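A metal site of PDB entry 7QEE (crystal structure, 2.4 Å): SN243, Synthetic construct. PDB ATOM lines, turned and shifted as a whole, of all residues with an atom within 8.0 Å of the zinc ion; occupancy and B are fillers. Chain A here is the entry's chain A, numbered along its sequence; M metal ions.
O of Glu 37 binds the zinc ion, at 2.1 Å.
OE1 of Glu 42 binds the zinc ion, 2.2 Å away.
The side-chain amide oxygen (OD1) of Asn 33 is bound to the zinc ion (2.5 Å).
The zinc ion has three donor atoms within binding distance.
Slightly farther from the zinc ion lies OE2 of Glu 42 (2.6 Å).
Slightly farther from the zinc ion lies the side-chain amide oxygen (OD1) of Asn 35 (2.7 Å).
Slightly farther from the zinc ion lies OD1 of Asp 31 (2.7 Å).
Slightly farther from the zinc ion lies the side-chain carboxylate (OD1) of Asp 39 (2.8 Å).
The side-chain amide nitrogen (ND2) of Asn 35 lies close to the side-chain amide nitrogen (ND2) of Asn 33 (3.0 Å).
OH of Tyr 41 lies within hydrogen-bond range of N of Asn 33 (3.4 Å).
The side-chain amide oxygen of Asn 33 sits close to the side-chain carboxylate of Asp 31, at 2.8 Å.
The side-chain carboxylate of Asp 39 is in hydrogen-bond range of the side-chain amide nitrogen of Gln 58.
The side-chain carboxylate (OE1) of Glu 42 lies close to the backbone NH (N) of Asp 39 (2.7 Å).
OD1 of Asp 39 sits at hydrogen-bond distance from ND2 of Asn 35, at 3.0 Å.
The side-chain amide nitrogen (ND2) of Asn 33 sits at hydrogen-bond distance from the side-chain carboxylate (OD1) of Asp 39 (2.7 Å).
The backbone NH (N) of Glu 37 lies within hydrogen-bond range of the side-chain amide oxygen (OD1) of Asn 35 (3.0 Å).
Leu 38 touches the zinc ion (CA to ZN, 3.9 Å).
Of the 19 residues printed, 7 come within 4 Å of the zinc ion.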
ATOM      1  N   GLU A  20     -18.228  -9.434 -16.968  1.00  0.00           N
ATOM      2  CA  GLU A  20     -17.327 -10.451 -17.479  1.00  0.00           C
ATOM      3  C   GLU A  20     -15.996 -10.410 -16.738  1.00  0.00           C
ATOM      4  O   GLU A  20     -15.590  -9.366 -16.233  1.00  0.00           O
ATOM      5  CB  GLU A  20     -17.082 -10.255 -18.988  1.00  0.00           C
ATOM      6  CG  GLU A  20     -17.974 -11.084 -19.934  1.00  0.00           C
ATOM      7  CD  GLU A  20     -19.159 -10.290 -20.506  1.00  0.00           C
ATOM      8  OE1 GLU A  20     -19.238  -9.060 -20.277  1.00  0.00           O
ATOM      9  OE2 GLU A  20     -19.999 -10.895 -21.200  1.00  0.00           O
ATOM     10  N   ILE A  22     -11.770 -10.901 -16.891  1.00  0.00           N
ATOM     11  CA  ILE A  22     -10.767 -10.679 -17.910  1.00  0.00           C
ATOM     12  C   ILE A  22      -9.395 -11.042 -17.362  1.00  0.00           C
ATOM     13  O   ILE A  22      -9.075 -10.775 -16.192  1.00  0.00           O
ATOM     14  CB  ILE A  22     -10.724  -9.250 -18.482  1.00  0.00           C
ATOM     15  CG1 ILE A  22     -10.246  -8.243 -17.430  1.00  0.00           C
ATOM     16  CG2 ILE A  22     -12.044  -8.915 -19.144  1.00  0.00           C
ATOM     17  CD1 ILE A  22     -10.451  -6.794 -17.826  1.00  0.00           C
ATOM     18  N   PHE A  29      -9.429 -10.830 -13.197  1.00  0.00           N
ATOM     19  CA  PHE A  29      -9.986  -9.568 -12.732  1.00  0.00           C
ATOM     20  C   PHE A  29     -11.411  -9.444 -13.252  1.00  0.00           C
ATOM     21  O   PHE A  29     -11.741  -9.993 -14.301  1.00  0.00           O
ATOM     22  CB  PHE A  29      -9.162  -8.361 -13.232  1.00  0.00           C
ATOM     23  CG  PHE A  29      -7.691  -8.420 -12.867  1.00  0.00           C
ATOM     24  CD1 PHE A  29      -7.238  -7.926 -11.642  1.00  0.00           C
ATOM     25  CD2 PHE A  29      -6.765  -8.956 -13.744  1.00  0.00           C
ATOM     26  CE1 PHE A  29      -5.887  -7.982 -11.305  1.00  0.00           C
ATOM     27  CE2 PHE A  29      -5.410  -9.006 -13.413  1.00  0.00           C
ATOM     28  CZ  PHE A  29      -4.963  -8.517 -12.195  1.00  0.00           C
ATOM     29  N   ARG A  30     -12.241  -8.691 -12.531  1.00  0.00           N
ATOM     30  CA  ARG A  30     -13.618  -8.431 -12.957  1.00  0.00           C
ATOM     31  C   ARG A  30     -13.720  -7.125 -13.738  1.00  0.00           C
ATOM     32  O   ARG A  30     -13.288  -6.078 -13.258  1.00  0.00           O
ATOM     33  CB  ARG A  30     -14.569  -8.383 -11.773  1.00  0.00           C
ATOM     34  CG  ARG A  30     -14.763  -9.725 -11.116  1.00  0.00           C
ATOM     35  CD  ARG A  30     -15.402  -9.602  -9.745  1.00  0.00           C
ATOM     36  NE  ARG A  30     -16.867  -9.523  -9.803  1.00  0.00           N
ATOM     37  CZ  ARG A  30     -17.592  -8.789  -8.967  1.00  0.00           C
ATOM     38  NH1 ARG A  30     -18.914  -8.769  -9.067  1.00  0.00           N
ATOM     39  NH2 ARG A  30     -16.976  -8.084  -8.028  1.00  0.00           N
ATOM     40  N   ASP A  31     -14.333  -7.190 -14.926  1.00  0.00           N
ATOM     41  CA  ASP A  31     -14.476  -6.027 -15.801  1.00  0.00           C
ATOM     42  C   ASP A  31     -15.777  -5.287 -15.466  1.00  0.00           C
ATOM     43  O   ASP A  31     -16.779  -5.330 -16.187  1.00  0.00           O
ATOM     44  CB  ASP A  31     -14.452  -6.462 -17.262  1.00  0.00           C
ATOM     45  CG  ASP A  31     -14.761  -5.327 -18.222  1.00  0.00           C
ATOM     46  OD1 ASP A  31     -14.192  -4.241 -18.031  1.00  0.00           O
ATOM     47  OD2 ASP A  31     -15.570  -5.526 -19.162  1.00  0.00           O
ATOM     48  N   LEU A  32     -15.732  -4.576 -14.328  1.00  0.00           N
ATOM     49  CA  LEU A  32     -16.955  -4.071 -13.704  1.00  0.00           C
ATOM     50  C   LEU A  32     -17.578  -2.905 -14.458  1.00  0.00           C
ATOM     51  O   LEU A  32     -18.760  -2.609 -14.268  1.00  0.00           O
ATOM     52  CB  LEU A  32     -16.666  -3.684 -12.250  1.00  0.00           C
ATOM     53  CG  LEU A  32     -16.543  -4.845 -11.251  1.00  0.00           C
ATOM     54  CD1 LEU A  32     -15.827  -4.382 -10.019  1.00  0.00           C
ATOM     55  CD2 LEU A  32     -17.925  -5.366 -10.873  1.00  0.00           C
ATOM     56  N   ASN A  33     -16.790  -2.178 -15.254  1.00  0.00           N
ATOM     57  CA  ASN A  33     -17.302  -1.102 -16.087  1.00  0.00           C
ATOM     58  C   ASN A  33     -17.689  -1.568 -17.485  1.00  0.00           C
ATOM     59  O   ASN A  33     -18.113  -0.736 -18.295  1.00  0.00           O
ATOM     60  CB  ASN A  33     -16.265   0.010 -16.188  1.00  0.00           C
ATOM     61  CG  ASN A  33     -14.956  -0.472 -16.795  1.00  0.00           C
ATOM     62  OD1 ASN A  33     -14.856  -1.601 -17.297  1.00  0.00           O
ATOM     63  ND2 ASN A  33     -13.933   0.375 -16.723  1.00  0.00           N
ATOM     64  N   ASP A  34     -17.495  -2.866 -17.801  1.00  0.00           N
ATOM     65  CA  ASP A  34     -17.904  -3.457 -19.075  1.00  0.00           C
ATOM     66  C   ASP A  34     -17.188  -2.785 -20.247  1.00  0.00           C
ATOM     67  O   ASP A  34     -17.750  -2.651 -21.334  1.00  0.00           O
ATOM     68  CB  ASP A  34     -19.419  -3.428 -19.298  1.00  0.00           C
ATOM     69  CG  ASP A  34     -19.901  -4.549 -20.250  1.00  0.00           C
ATOM     70  OD1 ASP A  34     -19.136  -5.531 -20.442  1.00  0.00           O
ATOM     71  OD2 ASP A  34     -21.018  -4.444 -20.812  1.00  0.00           O
ATOM     72  N   ASN A  35     -15.978  -2.275 -20.002  1.00  0.00           N
ATOM     73  CA  ASN A  35     -15.218  -1.617 -21.059  1.00  0.00           C
ATOM     74  C   ASN A  35     -14.182  -2.530 -21.695  1.00  0.00           C
ATOM     75  O   ASN A  35     -13.398  -2.052 -22.527  1.00  0.00           O
ATOM     76  CB  ASN A  35     -14.572  -0.337 -20.535  1.00  0.00           C
ATOM     77  CG  ASN A  35     -13.350  -0.600 -19.695  1.00  0.00           C
ATOM     78  OD1 ASN A  35     -13.054  -1.727 -19.354  1.00  0.00           O
ATOM     79  ND2 ASN A  35     -12.605   0.456 -19.379  1.00  0.00           N
ATOM     80  N   GLY A  36     -14.102  -3.784 -21.296  1.00  0.00           N
ATOM     81  CA  GLY A  36     -13.199  -4.716 -21.928  1.00  0.00           C
ATOM     82  C   GLY A  36     -11.748  -4.617 -21.524  1.00  0.00           C
ATOM     83  O   GLY A  36     -10.988  -5.564 -21.773  1.00  0.00           O
ATOM     84  N   GLU A  37     -11.323  -3.499 -20.957  1.00  0.00           N
ATOM     85  CA  GLU A  37      -9.971  -3.398 -20.426  1.00  0.00           C
ATOM     86  C   GLU A  37     -10.009  -3.239 -18.908  1.00  0.00           C
ATOM     87  O   GLU A  37     -11.040  -2.941 -18.304  1.00  0.00           O
ATOM     88  CB  GLU A  37      -9.198  -2.269 -21.112  1.00  0.00           C
ATOM     89  CG  GLU A  37      -9.319  -2.335 -22.637  1.00  0.00           C
ATOM     90  CD  GLU A  37      -8.102  -2.961 -23.325  1.00  0.00           C
ATOM     91  OE1 GLU A  37      -8.182  -3.247 -24.542  1.00  0.00           O
ATOM     92  OE2 GLU A  37      -7.079  -3.197 -22.651  1.00  0.00           O
ATOM     93  N   LEU A  38      -8.860  -3.445 -18.272  1.00  0.00           N
ATOM     94  CA  LEU A  38      -8.772  -3.471 -16.814  1.00  0.00           C
ATOM     95  C   LEU A  38      -8.441  -2.086 -16.269  1.00  0.00           C
ATOM     96  O   LEU A  38      -7.321  -1.595 -16.462  1.00  0.00           O
ATOM     97  CB  LEU A  38      -7.729  -4.504 -16.388  1.00  0.00           C
ATOM     98  CG  LEU A  38      -7.263  -4.438 -14.938  1.00  0.00           C
ATOM     99  CD1 LEU A  38      -8.330  -5.014 -14.032  1.00  0.00           C
ATOM    100  CD2 LEU A  38      -5.958  -5.180 -14.760  1.00  0.00           C
ATOM    101  N   ASP A  39      -9.409  -1.444 -15.586  1.00  0.00           N
ATOM    102  CA  ASP A  39      -9.176  -0.189 -14.864  1.00  0.00           C
ATOM    103  C   ASP A  39      -8.426  -0.417 -13.561  1.00  0.00           C
ATOM    104  O   ASP A  39      -8.443  -1.518 -12.991  1.00  0.00           O
ATOM    105  CB  ASP A  39     -10.480   0.522 -14.564  1.00  0.00           C
ATOM    106  CG  ASP A  39     -11.230   0.896 -15.803  1.00  0.00           C
ATOM    107  OD1 ASP A  39     -11.256   0.081 -16.744  1.00  0.00           O
ATOM    108  OD2 ASP A  39     -11.817   2.001 -15.834  1.00  0.00           O
ATOM    109  N   PRO A  40      -7.739   0.616 -13.051  1.00  0.00           N
ATOM    110  CA  PRO A  40      -7.109   0.490 -11.717  1.00  0.00           C
ATOM    111  C   PRO A  40      -8.057   0.067 -10.605  1.00  0.00           C
ATOM    112  O   PRO A  40      -7.653  -0.693  -9.713  1.00  0.00           O
ATOM    113  CB  PRO A  40      -6.552   1.896 -11.473  1.00  0.00           C
ATOM    114  CG  PRO A  40      -6.297   2.440 -12.833  1.00  0.00           C
ATOM    115  CD  PRO A  40      -7.386   1.881 -13.715  1.00  0.00           C
ATOM    116  N   TYR A  41      -9.317   0.541 -10.626  1.00  0.00           N
ATOM    117  CA  TYR A  41     -10.238   0.203  -9.546  1.00  0.00           C
ATOM    118  C   TYR A  41     -10.681  -1.257  -9.591  1.00  0.00           C
ATOM    119  O   TYR A  41     -11.102  -1.802  -8.573  1.00  0.00           O
ATOM    120  CB  TYR A  41     -11.432   1.159  -9.545  1.00  0.00           C
ATOM    121  CG  TYR A  41     -12.623   0.782 -10.370  1.00  0.00           C
ATOM    122  CD1 TYR A  41     -13.656   0.038  -9.819  1.00  0.00           C
ATOM    123  CD2 TYR A  41     -12.768   1.230 -11.669  1.00  0.00           C
ATOM    124  CE1 TYR A  41     -14.787  -0.297 -10.559  1.00  0.00           C
ATOM    125  CE2 TYR A  41     -13.900   0.895 -12.423  1.00  0.00           C
ATOM    126  CZ  TYR A  41     -14.903   0.137 -11.855  1.00  0.00           C
ATOM    127  OH  TYR A  41     -16.032  -0.197 -12.581  1.00  0.00           O
ATOM    128  N   GLU A  42     -10.613  -1.890 -10.765  1.00  0.00           N
ATOM    129  CA  GLU A  42     -10.842  -3.315 -10.896  1.00  0.00           C
ATOM    130  C   GLU A  42      -9.579  -4.141 -10.613  1.00  0.00           C
ATOM    131  O   GLU A  42      -9.648  -5.381 -10.616  1.00  0.00           O
ATOM    132  CB  GLU A  42     -11.369  -3.620 -12.296  1.00  0.00           C
ATOM    133  CG  GLU A  42     -12.646  -2.846 -12.649  1.00  0.00           C
ATOM    134  CD  GLU A  42     -12.792  -2.631 -14.155  1.00  0.00           C
ATOM    135  OE1 GLU A  42     -11.740  -2.625 -14.847  1.00  0.00           O
ATOM    136  OE2 GLU A  42     -13.939  -2.464 -14.635  1.00  0.00           O
ATOM    137  N   ASP A  43      -8.442  -3.498 -10.373  1.00  0.00           N
ATOM    138  CA  ASP A  43      -7.151  -4.170 -10.243  1.00  0.00           C
ATOM    139  C   ASP A  43      -6.863  -4.414  -8.770  1.00  0.00           C
ATOM    140  O   ASP A  43      -6.286  -3.573  -8.081  1.00  0.00           O
ATOM    141  CB  ASP A  43      -6.063  -3.327 -10.908  1.00  0.00           C
ATOM    142  CG  ASP A  43      -4.714  -4.016 -10.922  1.00  0.00           C
ATOM    143  OD1 ASP A  43      -4.366  -4.702  -9.936  1.00  0.00           O
ATOM    144  OD2 ASP A  43      -3.998  -3.888 -11.931  1.00  0.00           O
ATOM    145  N   ASP A  54      -9.207   6.025  -8.631  1.00  0.00           N
ATOM    146  CA  ASP A  54      -9.579   5.731 -10.016  1.00  0.00           C
ATOM    147  C   ASP A  54     -11.091   5.581 -10.169  1.00  0.00           C
ATOM    148  O   ASP A  54     -11.647   5.877 -11.241  1.00  0.00           O
ATOM    149  CB  ASP A  54      -8.865   4.491 -10.523  1.00  0.00           C
ATOM    150  CG  ASP A  54      -9.154   4.231 -11.991  1.00  0.00           C
ATOM    151  OD1 ASP A  54      -8.437   4.760 -12.857  1.00  0.00           O
ATOM    152  OD2 ASP A  54     -10.137   3.529 -12.281  1.00  0.00           O
ATOM    153  N   GLN A  58     -14.317   8.289 -12.249  1.00  0.00           N
ATOM    154  CA  GLN A  58     -15.239   7.896 -13.303  1.00  0.00           C
ATOM    155  C   GLN A  58     -16.710   8.035 -12.925  1.00  0.00           C
ATOM    156  O   GLN A  58     -17.564   7.546 -13.674  1.00  0.00           O
ATOM    157  CB  GLN A  58     -14.971   6.448 -13.693  1.00  0.00           C
ATOM    158  CG  GLN A  58     -13.518   6.108 -13.841  1.00  0.00           C
ATOM    159  CD  GLN A  58     -13.326   4.632 -14.129  1.00  0.00           C
ATOM    160  OE1 GLN A  58     -14.149   4.013 -14.812  1.00  0.00           O
ATOM    161  NE2 GLN A  58     -12.232   4.070 -13.630  1.00  0.00           N
HETATM  162 ZN    ZN M   1     -12.513  -2.434 -16.847  1.00  0.00          ZN
